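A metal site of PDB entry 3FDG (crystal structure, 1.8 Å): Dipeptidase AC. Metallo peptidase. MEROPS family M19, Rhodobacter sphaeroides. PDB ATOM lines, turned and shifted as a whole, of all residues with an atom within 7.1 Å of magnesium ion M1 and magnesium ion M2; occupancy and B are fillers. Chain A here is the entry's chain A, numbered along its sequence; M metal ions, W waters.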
ATOM      1  N   HIS A  11      -7.351 -14.171 -21.092  1.00  0.00           N
ATOM      2  CA  HIS A  11      -7.602 -15.616 -20.827  1.00  0.00           C
ATOM      3  C   HIS A  11      -6.318 -16.412 -20.701  1.00  0.00           C
ATOM      4  O   HIS A  11      -5.518 -16.453 -21.630  1.00  0.00           O
ATOM      5  CB  HIS A  11      -8.393 -16.273 -21.996  1.00  0.00           C
ATOM      6  CG  HIS A  11      -8.844 -17.692 -21.713  1.00  0.00           C
ATOM      7  ND1 HIS A  11     -10.062 -17.970 -21.156  1.00  0.00           N
ATOM      8  CD2 HIS A  11      -8.255 -18.889 -21.984  1.00  0.00           C
ATOM      9  CE1 HIS A  11     -10.217 -19.289 -21.063  1.00  0.00           C
ATOM     10  NE2 HIS A  11      -9.136 -19.870 -21.554  1.00  0.00           N
ATOM     11  N   ASN A  12      -6.158 -17.118 -19.580  1.00  0.00           N
ATOM     12  CA  ASN A  12      -5.119 -18.142 -19.523  1.00  0.00           C
ATOM     13  C   ASN A  12      -5.613 -19.354 -18.776  1.00  0.00           C
ATOM     14  O   ASN A  12      -6.560 -19.265 -17.964  1.00  0.00           O
ATOM     15  CB  ASN A  12      -3.840 -17.576 -18.859  1.00  0.00           C
ATOM     16  CG  ASN A  12      -4.051 -17.182 -17.401  1.00  0.00           C
ATOM     17  OD1 ASN A  12      -4.842 -17.830 -16.652  1.00  0.00           O
ATOM     18  ND2 ASN A  12      -3.386 -16.122 -16.983  1.00  0.00           N
ATOM     19  N   ASP A  13      -4.921 -20.480 -18.991  1.00  0.00           N
ATOM     20  CA  ASP A  13      -5.299 -21.768 -18.384  1.00  0.00           C
ATOM     21  C   ASP A  13      -4.198 -22.275 -17.475  1.00  0.00           C
ATOM     22  O   ASP A  13      -3.969 -23.499 -17.318  1.00  0.00           O
ATOM     23  CB  ASP A  13      -5.597 -22.786 -19.530  1.00  0.00           C
ATOM     24  CG  ASP A  13      -6.925 -22.444 -20.285  1.00  0.00           C
ATOM     25  OD1 ASP A  13      -8.036 -22.470 -19.676  1.00  0.00           O
ATOM     26  OD2 ASP A  13      -6.857 -22.096 -21.475  1.00  0.00           O
ATOM     27  N   LEU A  16      -4.955 -25.055 -15.004  1.00  0.00           N
ATOM     28  CA  LEU A  16      -5.070 -26.423 -15.440  1.00  0.00           C
ATOM     29  C   LEU A  16      -3.757 -27.123 -15.099  1.00  0.00           C
ATOM     30  O   LEU A  16      -3.732 -28.330 -14.770  1.00  0.00           O
ATOM     31  CB  LEU A  16      -5.428 -26.425 -16.939  1.00  0.00           C
ATOM     32  CG  LEU A  16      -5.837 -27.760 -17.556  1.00  0.00           C
ATOM     33  CD1 LEU A  16      -7.063 -28.370 -16.853  1.00  0.00           C
ATOM     34  CD2 LEU A  16      -6.081 -27.508 -19.076  1.00  0.00           C
ATOM     35  N   ALA A  54      -8.836 -18.781 -16.061  1.00  0.00           N
ATOM     36  CA  ALA A  54     -10.002 -19.686 -16.357  1.00  0.00           C
ATOM     37  C   ALA A  54     -10.005 -20.906 -15.474  1.00  0.00           C
ATOM     38  O   ALA A  54      -8.994 -21.626 -15.374  1.00  0.00           O
ATOM     39  CB  ALA A  54      -9.882 -20.181 -17.784  1.00  0.00           C
ATOM     40  N   ILE A  55     -11.181 -21.174 -14.920  1.00  0.00           N
ATOM     41  CA  ILE A  55     -11.579 -22.457 -14.419  1.00  0.00           C
ATOM     42  C   ILE A  55     -12.220 -23.156 -15.615  1.00  0.00           C
ATOM     43  O   ILE A  55     -13.282 -22.753 -16.120  1.00  0.00           O
ATOM     44  CB  ILE A  55     -12.573 -22.343 -13.265  1.00  0.00           C
ATOM     45  CG1 ILE A  55     -11.901 -21.634 -12.073  1.00  0.00           C
ATOM     46  CG2 ILE A  55     -13.125 -23.753 -12.865  1.00  0.00           C
ATOM     47  CD1 ILE A  55     -12.876 -21.124 -11.000  1.00  0.00           C
ATOM     48  N   TYR A  56     -11.554 -24.217 -16.055  1.00  0.00           N
ATOM     49  CA  TYR A  56     -11.992 -24.979 -17.218  1.00  0.00           C
ATOM     50  C   TYR A  56     -11.911 -26.476 -16.881  1.00  0.00           C
ATOM     51  O   TYR A  56     -10.824 -26.987 -16.535  1.00  0.00           O
ATOM     52  CB  TYR A  56     -11.135 -24.613 -18.432  1.00  0.00           C
ATOM     53  CG  TYR A  56     -11.085 -25.688 -19.462  1.00  0.00           C
ATOM     54  CD1 TYR A  56     -12.214 -25.981 -20.211  1.00  0.00           C
ATOM     55  CD2 TYR A  56      -9.926 -26.465 -19.629  1.00  0.00           C
ATOM     56  CE1 TYR A  56     -12.209 -27.011 -21.148  1.00  0.00           C
ATOM     57  CE2 TYR A  56      -9.911 -27.503 -20.577  1.00  0.00           C
ATOM     58  CZ  TYR A  56     -11.046 -27.744 -21.320  1.00  0.00           C
ATOM     59  OH  TYR A  56     -11.070 -28.746 -22.240  1.00  0.00           O
ATOM     60  N   HIS A 135     -12.548 -16.688 -13.593  1.00  0.00           N
ATOM     61  CA  HIS A 135     -13.305 -16.866 -14.813  1.00  0.00           C
ATOM     62  C   HIS A 135     -13.636 -18.343 -14.949  1.00  0.00           C
ATOM     63  O   HIS A 135     -12.844 -19.213 -14.552  1.00  0.00           O
ATOM     64  CB  HIS A 135     -12.483 -16.434 -16.030  1.00  0.00           C
ATOM     65  CG  HIS A 135     -13.140 -16.722 -17.349  1.00  0.00           C
ATOM     66  ND1 HIS A 135     -12.784 -17.774 -18.180  1.00  0.00           N
ATOM     67  CD2 HIS A 135     -14.120 -16.059 -17.983  1.00  0.00           C
ATOM     68  CE1 HIS A 135     -13.548 -17.767 -19.256  1.00  0.00           C
ATOM     69  NE2 HIS A 135     -14.366 -16.720 -19.165  1.00  0.00           N
ATOM     70  N   GLU A 137     -14.732 -21.165 -17.816  1.00  0.00           N
ATOM     71  CA  GLU A 137     -14.806 -21.371 -19.286  1.00  0.00           C
ATOM     72  C   GLU A 137     -15.642 -22.610 -19.517  1.00  0.00           C
ATOM     73  O   GLU A 137     -15.148 -23.738 -19.311  1.00  0.00           O
ATOM     74  CB  GLU A 137     -13.365 -21.553 -19.831  1.00  0.00           C
ATOM     75  CG  GLU A 137     -13.271 -21.956 -21.336  1.00  0.00           C
ATOM     76  CD  GLU A 137     -11.868 -21.910 -21.927  1.00  0.00           C
ATOM     77  OE1 GLU A 137     -10.876 -22.101 -21.224  1.00  0.00           O
ATOM     78  OE2 GLU A 137     -11.728 -21.685 -23.139  1.00  0.00           O
ATOM     79  N   TRP A 164     -17.709 -24.260 -23.475  1.00  0.00           N
ATOM     80  CA  TRP A 164     -16.426 -24.483 -24.092  1.00  0.00           C
ATOM     81  C   TRP A 164     -16.822 -25.160 -25.424  1.00  0.00           C
ATOM     82  O   TRP A 164     -18.000 -25.027 -25.891  1.00  0.00           O
ATOM     83  CB  TRP A 164     -15.542 -25.413 -23.176  1.00  0.00           C
ATOM     84  CG  TRP A 164     -14.195 -25.702 -23.797  1.00  0.00           C
ATOM     85  CD1 TRP A 164     -13.200 -24.778 -24.074  1.00  0.00           C
ATOM     86  CD2 TRP A 164     -13.705 -26.967 -24.259  1.00  0.00           C
ATOM     87  NE1 TRP A 164     -12.132 -25.427 -24.706  1.00  0.00           N
ATOM     88  CE2 TRP A 164     -12.414 -26.753 -24.797  1.00  0.00           C
ATOM     89  CE3 TRP A 164     -14.224 -28.270 -24.254  1.00  0.00           C
ATOM     90  CZ2 TRP A 164     -11.628 -27.799 -25.335  1.00  0.00           C
ATOM     91  CZ3 TRP A 164     -13.429 -29.316 -24.791  1.00  0.00           C
ATOM     92  CH2 TRP A 164     -12.162 -29.053 -25.347  1.00  0.00           C
ATOM     93  N   SER A 165     -15.888 -25.850 -26.073  1.00  0.00           N
ATOM     94  CA  SER A 165     -16.160 -26.467 -27.382  1.00  0.00           C
ATOM     95  C   SER A 165     -16.693 -27.870 -27.072  1.00  0.00           C
ATOM     96  O   SER A 165     -15.966 -28.863 -27.218  1.00  0.00           O
ATOM     97  CB  SER A 165     -14.883 -26.405 -28.256  1.00  0.00           C
ATOM     98  OG  SER A 165     -14.781 -25.095 -28.919  1.00  0.00           O
ATOM     99  N   PHE A 176     -13.782 -27.578 -33.019  1.00  0.00           N
ATOM    100  CA  PHE A 176     -12.605 -27.019 -33.659  1.00  0.00           C
ATOM    101  C   PHE A 176     -12.546 -27.537 -35.100  1.00  0.00           C
ATOM    102  O   PHE A 176     -12.515 -28.742 -35.318  1.00  0.00           O
ATOM    103  CB  PHE A 176     -11.342 -27.454 -32.931  1.00  0.00           C
ATOM    104  CG  PHE A 176     -11.329 -27.027 -31.480  1.00  0.00           C
ATOM    105  CD1 PHE A 176     -11.217 -25.662 -31.130  1.00  0.00           C
ATOM    106  CD2 PHE A 176     -11.472 -27.978 -30.462  1.00  0.00           C
ATOM    107  CE1 PHE A 176     -11.269 -25.256 -29.766  1.00  0.00           C
ATOM    108  CE2 PHE A 176     -11.514 -27.595 -29.126  1.00  0.00           C
ATOM    109  CZ  PHE A 176     -11.392 -26.231 -28.775  1.00  0.00           C
ATOM    110  N   ASP A 207     -18.784 -14.396 -21.490  1.00  0.00           N
ATOM    111  CA  ASP A 207     -17.688 -14.548 -22.454  1.00  0.00           C
ATOM    112  C   ASP A 207     -18.213 -15.401 -23.614  1.00  0.00           C
ATOM    113  O   ASP A 207     -18.667 -16.544 -23.401  1.00  0.00           O
ATOM    114  CB  ASP A 207     -16.434 -15.150 -21.792  1.00  0.00           C
ATOM    115  CG  ASP A 207     -15.303 -15.406 -22.796  1.00  0.00           C
ATOM    116  OD1 ASP A 207     -15.410 -14.945 -23.948  1.00  0.00           O
ATOM    117  OD2 ASP A 207     -14.300 -16.090 -22.453  1.00  0.00           O
ATOM    118  N   SER A 209     -16.505 -16.431 -26.360  1.00  0.00           N
ATOM    119  CA  SER A 209     -15.494 -17.285 -27.001  1.00  0.00           C
ATOM    120  C   SER A 209     -15.921 -18.741 -26.802  1.00  0.00           C
ATOM    121  O   SER A 209     -16.298 -19.146 -25.707  1.00  0.00           O
ATOM    122  CB  SER A 209     -14.063 -17.062 -26.442  1.00  0.00           C
ATOM    123  OG  SER A 209     -13.563 -15.761 -26.821  1.00  0.00           O
ATOM    124  N   HIS A 210     -15.811 -19.497 -27.882  1.00  0.00           N
ATOM    125  CA  HIS A 210     -16.288 -20.915 -28.014  1.00  0.00           C
ATOM    126  C   HIS A 210     -17.762 -21.037 -28.333  1.00  0.00           C
ATOM    127  O   HIS A 210     -18.237 -22.077 -28.840  1.00  0.00           O
ATOM    128  CB  HIS A 210     -15.991 -21.794 -26.776  1.00  0.00           C
ATOM    129  CG  HIS A 210     -14.528 -22.021 -26.550  1.00  0.00           C
ATOM    130  ND1 HIS A 210     -13.832 -23.028 -27.191  1.00  0.00           N
ATOM    131  CD2 HIS A 210     -13.632 -21.350 -25.789  1.00  0.00           C
ATOM    132  CE1 HIS A 210     -12.560 -22.975 -26.822  1.00  0.00           C
ATOM    133  NE2 HIS A 210     -12.423 -21.998 -25.940  1.00  0.00           N
ATOM    134  N   THR A 230     -13.373 -13.165 -25.005  1.00  0.00           N
ATOM    135  CA  THR A 230     -12.062 -12.948 -24.346  1.00  0.00           C
ATOM    136  C   THR A 230     -10.883 -13.493 -25.121  1.00  0.00           C
ATOM    137  O   THR A 230      -9.748 -13.049 -24.894  1.00  0.00           O
ATOM    138  CB  THR A 230     -12.023 -13.615 -22.940  1.00  0.00           C
ATOM    139  OG1 THR A 230     -12.208 -15.044 -23.086  1.00  0.00           O
ATOM    140  CG2 THR A 230     -13.111 -13.030 -22.014  1.00  0.00           C
ATOM    141  N   HIS A 231     -11.117 -14.443 -26.006  1.00  0.00           N
ATOM    142  CA  HIS A 231      -9.987 -15.025 -26.725  1.00  0.00           C
ATOM    143  C   HIS A 231     -10.366 -15.548 -28.110  1.00  0.00           C
ATOM    144  O   HIS A 231     -10.416 -16.769 -28.333  1.00  0.00           O
ATOM    145  CB  HIS A 231      -9.134 -16.013 -25.852  1.00  0.00           C
ATOM    146  CG  HIS A 231      -9.862 -17.244 -25.328  1.00  0.00           C
ATOM    147  ND1 HIS A 231     -10.963 -17.181 -24.510  1.00  0.00           N
ATOM    148  CD2 HIS A 231      -9.576 -18.556 -25.458  1.00  0.00           C
ATOM    149  CE1 HIS A 231     -11.335 -18.407 -24.156  1.00  0.00           C
ATOM    150  NE2 HIS A 231     -10.493 -19.263 -24.700  1.00  0.00           N
ATOM    151  N   ARG A 242     -13.580 -20.928 -34.601  1.00  0.00           N
ATOM    152  CA  ARG A 242     -13.395 -20.275 -33.290  1.00  0.00           C
ATOM    153  C   ARG A 242     -13.289 -18.732 -33.412  1.00  0.00           C
ATOM    154  O   ARG A 242     -13.347 -18.012 -32.391  1.00  0.00           O
ATOM    155  CB  ARG A 242     -12.130 -20.843 -32.605  1.00  0.00           C
ATOM    156  CG  ARG A 242     -12.392 -22.071 -31.753  1.00  0.00           C
ATOM    157  CD  ARG A 242     -13.059 -21.605 -30.439  1.00  0.00           C
ATOM    158  NE  ARG A 242     -12.125 -21.089 -29.439  1.00  0.00           N
ATOM    159  CZ  ARG A 242     -12.012 -19.806 -29.062  1.00  0.00           C
ATOM    160  NH1 ARG A 242     -12.725 -18.801 -29.660  1.00  0.00           N
ATOM    161  NH2 ARG A 242     -11.156 -19.526 -28.073  1.00  0.00           N
ATOM    162  N   ASN A 262      -6.353 -13.908 -29.449  1.00  0.00           N
ATOM    163  CA  ASN A 262      -5.881 -15.243 -29.058  1.00  0.00           C
ATOM    164  C   ASN A 262      -4.554 -15.486 -29.751  1.00  0.00           C
ATOM    165  O   ASN A 262      -4.397 -15.206 -30.975  1.00  0.00           O
ATOM    166  CB  ASN A 262      -6.950 -16.251 -29.536  1.00  0.00           C
ATOM    167  CG  ASN A 262      -6.806 -17.652 -28.896  1.00  0.00           C
ATOM    168  OD1 ASN A 262      -5.709 -18.176 -28.797  1.00  0.00           O
ATOM    169  ND2 ASN A 262      -7.953 -18.297 -28.577  1.00  0.00           N
ATOM    170  N   PHE A 267      -5.439 -20.045 -34.766  1.00  0.00           N
ATOM    171  CA  PHE A 267      -6.439 -18.974 -35.004  1.00  0.00           C
ATOM    172  C   PHE A 267      -5.851 -17.680 -35.598  1.00  0.00           C
ATOM    173  O   PHE A 267      -6.587 -16.723 -35.855  1.00  0.00           O
ATOM    174  CB  PHE A 267      -7.237 -18.668 -33.725  1.00  0.00           C
ATOM    175  CG  PHE A 267      -7.807 -19.896 -33.045  1.00  0.00           C
ATOM    176  CD1 PHE A 267      -8.258 -21.009 -33.784  1.00  0.00           C
ATOM    177  CD2 PHE A 267      -7.904 -19.911 -31.676  1.00  0.00           C
ATOM    178  CE1 PHE A 267      -8.778 -22.136 -33.129  1.00  0.00           C
ATOM    179  CE2 PHE A 267      -8.434 -21.016 -30.993  1.00  0.00           C
ATOM    180  CZ  PHE A 267      -8.837 -22.155 -31.725  1.00  0.00           C
ATOM    181  N   ASP A 304      -4.599 -16.933 -24.284  1.00  0.00           N
ATOM    182  CA  ASP A 304      -4.793 -18.405 -24.234  1.00  0.00           C
ATOM    183  C   ASP A 304      -3.430 -18.998 -23.779  1.00  0.00           C
ATOM    184  O   ASP A 304      -3.099 -20.167 -24.059  1.00  0.00           O
ATOM    185  CB  ASP A 304      -5.278 -18.954 -25.587  1.00  0.00           C
ATOM    186  CG  ASP A 304      -6.378 -20.064 -25.435  1.00  0.00           C
ATOM    187  OD1 ASP A 304      -6.730 -20.376 -24.307  1.00  0.00           O
ATOM    188  OD2 ASP A 304      -6.838 -20.650 -26.395  1.00  0.00           O
ATOM    189  N   PHE A 305      -2.662 -18.206 -23.046  1.00  0.00           N
ATOM    190  CA  PHE A 305      -1.390 -18.762 -22.430  1.00  0.00           C
ATOM    191  C   PHE A 305      -1.712 -20.064 -21.662  1.00  0.00           C
ATOM    192  O   PHE A 305      -2.753 -20.149 -20.980  1.00  0.00           O
ATOM    193  CB  PHE A 305      -0.779 -17.798 -21.457  1.00  0.00           C
ATOM    194  CG  PHE A 305       0.144 -16.755 -22.084  1.00  0.00           C
ATOM    195  CD1 PHE A 305       1.048 -17.106 -23.113  1.00  0.00           C
ATOM    196  CD2 PHE A 305       0.094 -15.408 -21.620  1.00  0.00           C
ATOM    197  CE1 PHE A 305       1.895 -16.091 -23.704  1.00  0.00           C
ATOM    198  CE2 PHE A 305       0.932 -14.452 -22.158  1.00  0.00           C
ATOM    199  CZ  PHE A 305       1.818 -14.764 -23.176  1.00  0.00           C
ATOM    200  N   ASP A 306      -0.876 -21.081 -21.815  1.00  0.00           N
ATOM    201  CA  ASP A 306      -1.083 -22.418 -21.247  1.00  0.00           C
ATOM    202  C   ASP A 306      -2.324 -23.177 -21.715  1.00  0.00           C
ATOM    203  O   ASP A 306      -2.649 -24.225 -21.140  1.00  0.00           O
ATOM    204  CB  ASP A 306      -0.981 -22.408 -19.699  1.00  0.00           C
ATOM    205  CG  ASP A 306       0.474 -22.237 -19.239  1.00  0.00           C
ATOM    206  OD1 ASP A 306       1.347 -22.827 -19.894  1.00  0.00           O
ATOM    207  OD2 ASP A 306       0.755 -21.504 -18.283  1.00  0.00           O
ATOM    208  N   GLY A 307      -3.000 -22.654 -22.741  1.00  0.00           N
ATOM    209  CA  GLY A 307      -4.153 -23.332 -23.342  1.00  0.00           C
ATOM    210  C   GLY A 307      -4.014 -23.559 -24.849  1.00  0.00           C
ATOM    211  O   GLY A 307      -4.943 -24.058 -25.421  1.00  0.00           O
HETATM  212 MG    MG M   1     -10.602 -21.568 -24.795  1.00  0.00          MG
HETATM  213 MG    MG M   2      -8.938 -22.003 -21.548  1.00  0.00          MG
HETATM  214  O   HOH W   1     -10.210 -23.979 -24.964  1.00  0.00           O
HETATM  215  O   HOH W   2      -8.714 -21.812 -23.660  1.00  0.00           O
HETATM  216  O   HOH W   3      -9.281 -21.659 -26.581  1.00  0.00           O
HETATM  217  O   HOH W   4      -9.149 -24.029 -21.955  1.00  0.00           O
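The backbone NH (N) of His 231 sits at hydrogen-bond distance from the side-chain hydroxyl (OG) of Ser 209, 2.9 Å away.
The backbone carbonyl oxygen of His 11 sits at hydrogen-bond distance from the backbone NH of Asp 304 (2.8 Å).
The guanidinium group (NH2) of Arg 242 lies close to the side-chain amide nitrogen (ND2) of Asn 262 (3.5 Å).
ND1 of His 231 is in hydrogen-bond range of OG1 of Thr 230 (2.9 Å).
ND2 of Asn 262 is in hydrogen-bond range of OD2 of Asp 304 (3.4 Å).
A ring nitrogen (ND1) of His 210 is in hydrogen-bond range of the side-chain hydroxyl (OG) of Ser 165 (2.9 Å).
A ring nitrogen (ND1) of His 210 lies close to the guanidinium group (NE) of Arg 242 (3.4 Å).
The backbone carbonyl oxygen (O) of Phe 305 sits at hydrogen-bond distance from the backbone NH (N) of Asp 13 (3.0 Å).
Merely in contact with magnesium ion M1: Arg 242 (3.9 Å).
Asp 304 touches magnesium ion M2.
Four residues have an atom within 4 Å of magnesium ion M2: His 11, Asp 13, Glu 137 and Asp 304.
OE2 of Glu 137 binds magnesium ion M1 (2.0 Å).
Magnesium ion M1 is bound by NE2 of His 210, 2.2 Å away.
Water W2 is bound to magnesium ion M1 (2.2 Å).
Water W3 binds magnesium ion M1 (2.2 Å).
NE2 of His 231 is bound to magnesium ion M1.
Magnesium ion M1 is bound by water W1.
Magnesium ion M1 has six donor atoms within binding distance.
Magnesium ion M2 is bound by the side-chain carboxylate (OE1) of Glu 137 (2.0 Å), water W4 (2.1 Å), the side-chain carboxylate (OD2) of Asp 13 (2.1 Å), the side-chain carboxylate (OD1) of Asp 13 (2.1 Å), water W2 (2.1 Å) and a ring nitrogen (NE2) of His 11 (2.1 Å).
Water W3 lies within hydrogen-bond range of OD2 of Asp 304 (2.6 Å) and NH2 of Arg 242 (3.2 Å).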
